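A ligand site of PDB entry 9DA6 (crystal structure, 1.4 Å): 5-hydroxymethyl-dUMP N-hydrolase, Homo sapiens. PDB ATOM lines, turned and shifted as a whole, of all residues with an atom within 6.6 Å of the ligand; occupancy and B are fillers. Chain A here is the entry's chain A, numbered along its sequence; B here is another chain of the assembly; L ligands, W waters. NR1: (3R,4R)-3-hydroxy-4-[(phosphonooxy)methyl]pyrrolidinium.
OG of Ser 111 of chain B sits at hydrogen-bond distance from O1 of the ligand (2.7 Å).
The side-chain carboxylate (OE2) of Glu 87 lies within salt-bridge range of a nitrogen (N1') of the ligand, at 2.7 Å.
The backbone NH of Arg 13 sits at hydrogen-bond distance from an oxygen (OP1) of the ligand.
The side-chain hydroxyl of Ser 81 is in hydrogen-bond range of an oxygen (OP2) of the ligand.
N of Ile 12 lies within hydrogen-bond range of OP2 of the ligand (2.9 Å).
N of Gly 83 is in hydrogen-bond range of O1 of the ligand (2.9 Å).
The backbone NH of Gly 14 lies within hydrogen-bond range of an oxygen (OP2) of the ligand, 2.9 Å away.
OD2 of Asp 63 is in salt-bridge range of N1' of the ligand (3.0 Å).
N of Gly 10 is in hydrogen-bond range of O3' of the ligand, 3.1 Å away.
An oxygen (O3') of the ligand lies close to the backbone carbonyl oxygen of Gly 10 (3.2 Å).
A nitrogen (N1') of the ligand is in salt-bridge range of the side-chain carboxylate of Glu 38, 3.6 Å away.
A nitrogen (N1') of the ligand lies close to the side-chain sulfur (SD) of Met 113 of chain B (3.8 Å).
OG of Ser 111 of chain B sits at hydrogen-bond distance from N of Gly 83 (3.4 Å).
OG of Ser 111 of chain B lies close to N of Met 113 of chain B (3.2 Å).
OE1 of Glu 87 sits close to SG of Cys 9 (3.4 Å).
OE2 of Glu 87 sits at hydrogen-bond distance from OH of Tyr 7, 2.6 Å away.
The side-chain hydroxyl (OG) of Ser 81 lies within hydrogen-bond range of the backbone NH (N) of Gly 83 (3.3 Å).
The backbone carbonyl oxygen (O) of Gly 10 lies within hydrogen-bond range of a ring nitrogen (NE2) of His 39, 2.9 Å away.
The side-chain hydroxyl (OG) of Ser 11 is in hydrogen-bond range of the backbone carbonyl oxygen (O) of Gly 15 (2.8 Å).
The side-chain hydroxyl of Thr 37 is in hydrogen-bond range of the backbone NH of His 39 (3.2 Å).
CA of Cys 9 touches O3' of the ligand, 3.3 Å away.
Ser 11 touches the ligand.
His 39 touches the ligand.
Val 84 touches the ligand.
Hydrophobic or aromatic side chains within 4 Å of the ligand: Ile 12 and Met 113 of chain B.
Water W1 lies within hydrogen-bond range of an oxygen (OP1) of the ligand (2.6 Å) and the backbone NH of Ala 112 of chain B (2.9 Å).
Water W4 bridges an oxygen (O1) of the ligand (2.8 Å) and the backbone NH (N) of Leu 82 (2.9 Å).
Water W2 lies within hydrogen-bond range of OH of Tyr 7 (2.8 Å), O of Phe 8 (2.9 Å), N of Glu 38 (2.9 Å), OG1 of Thr 37 (3.2 Å) and O3' of the ligand (3.4 Å).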
ATOM      1  N   TYR A   7       6.635 -14.305  -5.119  1.00  0.00           N
ATOM      2  CA  TYR A   7       5.425 -13.515  -4.950  1.00  0.00           C
ATOM      3  C   TYR A   7       5.476 -12.326  -5.901  1.00  0.00           C
ATOM      4  O   TYR A   7       6.493 -11.620  -5.929  1.00  0.00           O
ATOM      5  CB  TYR A   7       5.314 -13.036  -3.486  1.00  0.00           C
ATOM      6  CG  TYR A   7       4.003 -12.315  -3.234  1.00  0.00           C
ATOM      7  CD1 TYR A   7       2.854 -13.021  -2.943  1.00  0.00           C
ATOM      8  CD2 TYR A   7       3.909 -10.945  -3.371  1.00  0.00           C
ATOM      9  CE1 TYR A   7       1.646 -12.375  -2.768  1.00  0.00           C
ATOM     10  CE2 TYR A   7       2.681 -10.277  -3.202  1.00  0.00           C
ATOM     11  CZ  TYR A   7       1.567 -11.009  -2.886  1.00  0.00           C
ATOM     12  OH  TYR A   7       0.335 -10.435  -2.729  1.00  0.00           O
ATOM     13  N   PHE A   8       4.411 -12.090  -6.668  1.00  0.00           N
ATOM     14  CA  PHE A   8       4.374 -10.970  -7.602  1.00  0.00           C
ATOM     15  C   PHE A   8       3.422  -9.867  -7.129  1.00  0.00           C
ATOM     16  O   PHE A   8       2.247 -10.123  -6.887  1.00  0.00           O
ATOM     17  CB  PHE A   8       3.975 -11.384  -9.032  1.00  0.00           C
ATOM     18  CG  PHE A   8       3.848 -10.190  -9.955  1.00  0.00           C
ATOM     19  CD1 PHE A   8       4.975  -9.517 -10.366  1.00  0.00           C
ATOM     20  CD2 PHE A   8       2.608  -9.684 -10.263  1.00  0.00           C
ATOM     21  CE1 PHE A   8       4.857  -8.347 -11.130  1.00  0.00           C
ATOM     22  CE2 PHE A   8       2.496  -8.546 -11.043  1.00  0.00           C
ATOM     23  CZ  PHE A   8       3.605  -7.895 -11.460  1.00  0.00           C
ATOM     24  N   CYS A   9       3.955  -8.655  -7.017  1.00  0.00           N
ATOM     25  CA  CYS A   9       3.261  -7.432  -6.659  1.00  0.00           C
ATOM     26  C   CYS A   9       3.125  -6.473  -7.816  1.00  0.00           C
ATOM     27  O   CYS A   9       4.086  -6.232  -8.542  1.00  0.00           O
ATOM     28  CB  CYS A   9       3.920  -6.665  -5.491  1.00  0.00           C
ATOM     29  SG  CYS A   9       4.745  -7.527  -4.190  1.00  0.00           S
ATOM     30  N   GLY A  10       1.942  -5.883  -7.958  1.00  0.00           N
ATOM     31  CA  GLY A  10       1.731  -4.816  -8.937  1.00  0.00           C
ATOM     32  C   GLY A  10       0.398  -4.163  -8.645  1.00  0.00           C
ATOM     33  O   GLY A  10      -0.465  -4.756  -7.992  1.00  0.00           O
ATOM     34  N   SER A  11       0.245  -2.933  -9.156  1.00  0.00           N
ATOM     35  CA  SER A  11      -0.953  -2.164  -8.864  1.00  0.00           C
ATOM     36  C   SER A  11      -2.234  -2.851  -9.333  1.00  0.00           C
ATOM     37  O   SER A  11      -2.270  -3.450 -10.416  1.00  0.00           O
ATOM     38  CB  SER A  11      -0.823  -0.818  -9.563  1.00  0.00           C
ATOM     39  OG  SER A  11      -1.917   0.047  -9.274  1.00  0.00           O
ATOM     40  N   ILE A  12      -3.287  -2.744  -8.517  1.00  0.00           N
ATOM     41  CA  ILE A  12      -4.640  -3.149  -8.889  1.00  0.00           C
ATOM     42  C   ILE A  12      -5.574  -1.955  -8.660  1.00  0.00           C
ATOM     43  O   ILE A  12      -5.953  -1.268  -9.615  1.00  0.00           O
ATOM     44  CB  ILE A  12      -5.116  -4.427  -8.172  1.00  0.00           C
ATOM     45  CG1 ILE A  12      -4.148  -5.594  -8.474  1.00  0.00           C
ATOM     46  CG2 ILE A  12      -6.532  -4.789  -8.613  1.00  0.00           C
ATOM     47  CD1 ILE A  12      -4.469  -6.894  -7.714  1.00  0.00           C
ATOM     48  N   ARG A  13      -5.945  -1.689  -7.412  1.00  0.00           N
ATOM     49  CA  ARG A  13      -6.774  -0.532  -7.115  1.00  0.00           C
ATOM     50  C   ARG A  13      -6.046   0.797  -7.306  1.00  0.00           C
ATOM     51  O   ARG A  13      -6.712   1.827  -7.476  1.00  0.00           O
ATOM     52  CB  ARG A  13      -7.398  -0.651  -5.716  1.00  0.00           C
ATOM     53  CG  ARG A  13      -8.295  -1.882  -5.626  1.00  0.00           C
ATOM     54  CD  ARG A  13      -9.032  -1.968  -4.332  1.00  0.00           C
ATOM     55  NE  ARG A  13      -9.861  -3.171  -4.257  1.00  0.00           N
ATOM     56  CZ  ARG A  13     -10.411  -3.618  -3.143  1.00  0.00           C
ATOM     57  NH1 ARG A  13     -10.299  -2.958  -2.006  1.00  0.00           N
ATOM     58  NH2 ARG A  13     -11.083  -4.765  -3.161  1.00  0.00           N
ATOM     59  N   GLY A  14      -4.718   0.817  -7.295  1.00  0.00           N
ATOM     60  CA  GLY A  14      -4.022   2.018  -7.691  1.00  0.00           C
ATOM     61  C   GLY A  14      -4.159   2.329  -9.166  1.00  0.00           C
ATOM     62  O   GLY A  14      -3.826   3.450  -9.577  1.00  0.00           O
ATOM     63  N   GLY A  15      -4.627   1.375  -9.951  1.00  0.00           N
ATOM     64  CA  GLY A  15      -4.786   1.520 -11.382  1.00  0.00           C
ATOM     65  C   GLY A  15      -4.245   0.312 -12.100  1.00  0.00           C
ATOM     66  O   GLY A  15      -3.235  -0.260 -11.671  1.00  0.00           O
ATOM     67  N   THR A  37       0.329 -14.933  -6.386  1.00  0.00           N
ATOM     68  CA  THR A  37      -0.055 -13.562  -6.697  1.00  0.00           C
ATOM     69  C   THR A  37      -1.564 -13.471  -6.713  1.00  0.00           C
ATOM     70  O   THR A  37      -2.273 -14.434  -7.009  1.00  0.00           O
ATOM     71  CB  THR A  37       0.545 -13.149  -8.049  1.00  0.00           C
ATOM     72  OG1 THR A  37       0.314 -11.752  -8.284  1.00  0.00           O
ATOM     73  CG2 THR A  37      -0.046 -13.949  -9.198  1.00  0.00           C
ATOM     74  N   GLU A  38      -2.052 -12.275  -6.398  1.00  0.00           N
ATOM     75  CA  GLU A  38      -3.460 -11.959  -6.569  1.00  0.00           C
ATOM     76  C   GLU A  38      -3.788 -11.719  -8.039  1.00  0.00           C
ATOM     77  O   GLU A  38      -4.953 -11.812  -8.428  1.00  0.00           O
ATOM     78  CB  GLU A  38      -3.809 -10.740  -5.705  1.00  0.00           C
ATOM     79  CG  GLU A  38      -5.257 -10.286  -5.834  1.00  0.00           C
ATOM     80  CD  GLU A  38      -5.645  -9.125  -4.941  1.00  0.00           C
ATOM     81  OE1 GLU A  38      -4.847  -8.691  -4.093  1.00  0.00           O
ATOM     82  OE2 GLU A  38      -6.743  -8.597  -5.139  1.00  0.00           O
ATOM     83  N   HIS A  39      -2.775 -11.397  -8.861  1.00  0.00           N
ATOM     84  CA  HIS A  39      -2.989 -11.109 -10.268  1.00  0.00           C
ATOM     85  C   HIS A  39      -3.413 -12.362 -11.033  1.00  0.00           C
ATOM     86  O   HIS A  39      -2.824 -13.443 -10.850  1.00  0.00           O
ATOM     87  CB  HIS A  39      -1.730 -10.471 -10.875  1.00  0.00           C
ATOM     88  CG  HIS A  39      -1.423  -9.125 -10.298  1.00  0.00           C
ATOM     89  ND1 HIS A  39      -1.856  -7.969 -10.881  1.00  0.00           N
ATOM     90  CD2 HIS A  39      -0.750  -8.761  -9.171  1.00  0.00           C
ATOM     91  CE1 HIS A  39      -1.509  -6.942 -10.119  1.00  0.00           C
ATOM     92  NE2 HIS A  39      -0.812  -7.393  -9.094  1.00  0.00           N
ATOM     93  N   ILE A  59      -8.628 -10.652   1.484  1.00  0.00           N
ATOM     94  CA  ILE A  59      -7.580 -10.412   0.504  1.00  0.00           C
ATOM     95  C   ILE A  59      -6.253 -10.079   1.203  1.00  0.00           C
ATOM     96  O   ILE A  59      -5.198 -10.601   0.848  1.00  0.00           O
ATOM     97  CB  ILE A  59      -7.982  -9.287  -0.479  1.00  0.00           C
ATOM     98  CG1 ILE A  59      -9.191  -9.685  -1.303  1.00  0.00           C
ATOM     99  CG2 ILE A  59      -6.782  -8.917  -1.356  1.00  0.00           C
ATOM    100  CD1 ILE A  59      -9.834  -8.518  -2.014  1.00  0.00           C
ATOM    101  N   ASP A  63      -3.040 -12.483   0.710  1.00  0.00           N
ATOM    102  CA  ASP A  63      -1.839 -11.967   0.064  1.00  0.00           C
ATOM    103  C   ASP A  63      -0.673 -11.980   1.045  1.00  0.00           C
ATOM    104  O   ASP A  63       0.472 -12.294   0.658  1.00  0.00           O
ATOM    105  CB  ASP A  63      -2.107 -10.548  -0.435  1.00  0.00           C
ATOM    106  CG  ASP A  63      -3.003 -10.479  -1.682  1.00  0.00           C
ATOM    107  OD1 ASP A  63      -3.551 -11.507  -2.135  1.00  0.00           O
ATOM    108  OD2 ASP A  63      -3.135  -9.356  -2.247  1.00  0.00           O
ATOM    109  N   PRO A  80       2.047   4.018  -9.204  1.00  0.00           N
ATOM    110  CA  PRO A  80       1.973   4.172  -7.732  1.00  0.00           C
ATOM    111  C   PRO A  80       0.801   3.397  -7.152  1.00  0.00           C
ATOM    112  O   PRO A  80      -0.303   3.411  -7.695  1.00  0.00           O
ATOM    113  CB  PRO A  80       1.820   5.692  -7.554  1.00  0.00           C
ATOM    114  CG  PRO A  80       2.454   6.278  -8.772  1.00  0.00           C
ATOM    115  CD  PRO A  80       2.086   5.331  -9.882  1.00  0.00           C
ATOM    116  N   SER A  81       1.045   2.735  -6.021  1.00  0.00           N
ATOM    117  CA  SER A  81       0.053   1.848  -5.435  1.00  0.00           C
ATOM    118  C   SER A  81       0.333   1.688  -3.954  1.00  0.00           C
ATOM    119  O   SER A  81       1.448   1.336  -3.571  1.00  0.00           O
ATOM    120  CB  SER A  81       0.118   0.482  -6.107  1.00  0.00           C
ATOM    121  OG  SER A  81      -0.486  -0.529  -5.317  1.00  0.00           O
ATOM    122  N   LEU A  82      -0.689   1.934  -3.118  1.00  0.00           N
ATOM    123  CA  LEU A  82      -0.548   1.667  -1.688  1.00  0.00           C
ATOM    124  C   LEU A  82      -0.266   0.205  -1.411  1.00  0.00           C
ATOM    125  O   LEU A  82       0.546  -0.116  -0.546  1.00  0.00           O
ATOM    126  CB  LEU A  82      -1.802   2.078  -0.928  1.00  0.00           C
ATOM    127  CG  LEU A  82      -2.204   3.545  -0.977  1.00  0.00           C
ATOM    128  CD1 LEU A  82      -3.656   3.661  -0.510  1.00  0.00           C
ATOM    129  CD2 LEU A  82      -1.274   4.358  -0.142  1.00  0.00           C
ATOM    130  N   GLY A  83      -0.994  -0.705  -2.087  1.00  0.00           N
ATOM    131  CA  GLY A  83      -0.846  -2.107  -1.795  1.00  0.00           C
ATOM    132  C   GLY A  83       0.533  -2.635  -2.138  1.00  0.00           C
ATOM    133  O   GLY A  83       1.078  -3.469  -1.414  1.00  0.00           O
ATOM    134  N   VAL A  84       1.062  -2.234  -3.282  1.00  0.00           N
ATOM    135  CA  VAL A  84       2.413  -2.625  -3.650  1.00  0.00           C
ATOM    136  C   VAL A  84       3.426  -2.125  -2.630  1.00  0.00           C
ATOM    137  O   VAL A  84       4.289  -2.870  -2.161  1.00  0.00           O
ATOM    138  CB  VAL A  84       2.772  -2.109  -5.047  1.00  0.00           C
ATOM    139  CG1 VAL A  84       4.243  -2.394  -5.369  1.00  0.00           C
ATOM    140  CG2 VAL A  84       1.899  -2.785  -6.090  1.00  0.00           C
ATOM    141  N   GLY A  85       3.323  -0.857  -2.240  1.00  0.00           N
ATOM    142  CA  GLY A  85       4.224  -0.360  -1.234  1.00  0.00           C
ATOM    143  C   GLY A  85       4.116  -1.090   0.094  1.00  0.00           C
ATOM    144  O   GLY A  85       5.118  -1.365   0.740  1.00  0.00           O
ATOM    145  N   GLU A  87       3.086  -4.189   0.590  1.00  0.00           N
ATOM    146  CA  GLU A  87       3.702  -5.515   0.437  1.00  0.00           C
ATOM    147  C   GLU A  87       5.213  -5.427   0.524  1.00  0.00           C
ATOM    148  O   GLU A  87       5.861  -6.274   1.136  1.00  0.00           O
ATOM    149  CB  GLU A  87       3.231  -6.189  -0.856  1.00  0.00           C
ATOM    150  CG  GLU A  87       1.796  -6.640  -0.768  1.00  0.00           C
ATOM    151  CD  GLU A  87       1.205  -7.174  -2.060  1.00  0.00           C
ATOM    152  OE1 GLU A  87       1.638  -6.729  -3.143  1.00  0.00           O
ATOM    153  OE2 GLU A  87       0.249  -7.985  -1.954  1.00  0.00           O
ATOM    154  N   PRO B  80      -3.151   7.176  -4.293  1.00  0.00           N
ATOM    155  CA  PRO B  80      -2.275   5.997  -4.230  1.00  0.00           C
ATOM    156  C   PRO B  80      -0.809   6.401  -4.221  1.00  0.00           C
ATOM    157  O   PRO B  80      -0.392   7.310  -4.952  1.00  0.00           O
ATOM    158  CB  PRO B  80      -2.670   5.196  -5.487  1.00  0.00           C
ATOM    159  CG  PRO B  80      -4.098   5.613  -5.732  1.00  0.00           C
ATOM    160  CD  PRO B  80      -4.141   7.079  -5.378  1.00  0.00           C
ATOM    161  N   VAL B 109     -11.471   3.222  -4.984  1.00  0.00           N
ATOM    162  CA  VAL B 109     -11.628   2.138  -4.008  1.00  0.00           C
ATOM    163  C   VAL B 109     -10.297   1.979  -3.282  1.00  0.00           C
ATOM    164  O   VAL B 109      -9.264   1.745  -3.906  1.00  0.00           O
ATOM    165  CB  VAL B 109     -12.073   0.833  -4.679  1.00  0.00           C
ATOM    166  CG1 VAL B 109     -12.303  -0.265  -3.615  1.00  0.00           C
ATOM    167  CG2 VAL B 109     -13.327   1.064  -5.511  1.00  0.00           C
ATOM    168  N   LEU B 110     -10.319   2.097  -1.962  1.00  0.00           N
ATOM    169  CA  LEU B 110      -9.090   1.976  -1.186  1.00  0.00           C
ATOM    170  C   LEU B 110      -8.502   0.565  -1.315  1.00  0.00           C
ATOM    171  O   LEU B 110      -9.225  -0.429  -1.195  1.00  0.00           O
ATOM    172  CB  LEU B 110      -9.389   2.273   0.284  1.00  0.00           C
ATOM    173  CG  LEU B 110      -8.199   2.109   1.236  1.00  0.00           C
ATOM    174  CD1 LEU B 110      -7.031   2.999   0.937  1.00  0.00           C
ATOM    175  CD2 LEU B 110      -8.615   2.340   2.652  1.00  0.00           C
ATOM    176  N   SER B 111      -7.186   0.507  -1.540  1.00  0.00           N
ATOM    177  CA  SER B 111      -6.418  -0.738  -1.528  1.00  0.00           C
ATOM    178  C   SER B 111      -6.925  -1.735  -0.497  1.00  0.00           C
ATOM    179  O   SER B 111      -7.091  -1.389   0.674  1.00  0.00           O
ATOM    180  CB  SER B 111      -4.979  -0.411  -1.155  1.00  0.00           C
ATOM    181  OG  SER B 111      -4.165  -1.569  -1.160  1.00  0.00           O
ATOM    182  N   ALA B 112      -7.136  -2.979  -0.928  1.00  0.00           N
ATOM    183  CA  ALA B 112      -7.498  -4.023   0.025  1.00  0.00           C
ATOM    184  C   ALA B 112      -6.402  -4.250   1.072  1.00  0.00           C
ATOM    185  O   ALA B 112      -6.708  -4.687   2.184  1.00  0.00           O
ATOM    186  CB  ALA B 112      -7.802  -5.326  -0.717  1.00  0.00           C
ATOM    187  N   MET B 113      -5.152  -3.963   0.733  1.00  0.00           N
ATOM    188  CA  MET B 113      -4.083  -4.178   1.705  1.00  0.00           C
ATOM    189  C   MET B 113      -4.096  -3.177   2.840  1.00  0.00           C
ATOM    190  O   MET B 113      -3.536  -3.452   3.912  1.00  0.00           O
ATOM    191  CB  MET B 113      -2.719  -4.138   1.051  1.00  0.00           C
ATOM    192  CG  MET B 113      -2.505  -5.170  -0.020  1.00  0.00           C
ATOM    193  SD  MET B 113      -2.874  -6.886   0.447  1.00  0.00           S
ATOM    194  CE  MET B 113      -1.466  -7.268   1.521  1.00  0.00           C
ATOM    195  N   ILE B 114      -4.682  -2.007   2.612  1.00  0.00           N
ATOM    196  CA  ILE B 114      -4.841  -1.019   3.678  1.00  0.00           C
ATOM    197  C   ILE B 114      -6.151  -1.200   4.403  1.00  0.00           C
ATOM    198  O   ILE B 114      -6.189  -1.326   5.634  1.00  0.00           O
ATOM    199  CB  ILE B 114      -4.665   0.410   3.118  1.00  0.00           C
ATOM    200  CG1 ILE B 114      -3.341   0.565   2.389  1.00  0.00           C
ATOM    201  CG2 ILE B 114      -4.848   1.404   4.257  1.00  0.00           C
ATOM    202  CD1 ILE B 114      -2.096   0.096   3.143  1.00  0.00           C
HETATM  203  P   NR1 L   1      -3.490  -1.892  -4.837  1.00  0.00           P
HETATM  204  OP1 NR1 L   1      -4.814  -2.532  -5.060  1.00  0.00           O
HETATM  205  OP2 NR1 L   1      -3.024  -1.256  -6.093  1.00  0.00           O
HETATM  206  O5' NR1 L   1      -2.429  -3.085  -4.450  1.00  0.00           O
HETATM  207  C2' NR1 L   1      -1.932  -7.335  -4.589  1.00  0.00           C
HETATM  208  C5' NR1 L   1      -2.351  -4.234  -5.270  1.00  0.00           C
HETATM  209  C4' NR1 L   1      -1.176  -5.096  -4.746  1.00  0.00           C
HETATM  210  C3' NR1 L   1      -1.113  -6.387  -5.447  1.00  0.00           C
HETATM  211  C6' NR1 L   1      -1.366  -5.406  -3.269  1.00  0.00           C
HETATM  212  N1' NR1 L   1      -1.880  -6.826  -3.203  1.00  0.00           N
HETATM  213  O3' NR1 L   1       0.241  -6.806  -5.573  1.00  0.00           O
HETATM  214  O1  NR1 L   1      -3.432  -0.983  -3.686  1.00  0.00           O
HETATM  215  O   HOH W   1      -6.194  -4.038  -3.414  1.00  0.00           O
HETATM  216  O   HOH W   2      -0.251 -10.211  -5.482  1.00  0.00           O
HETATM  217  O   HOH W   3      -4.612  -6.245  -2.680  1.00  0.00           O
HETATM  218  O   HOH W   4      -3.408   1.804  -4.124  1.00  0.00           O
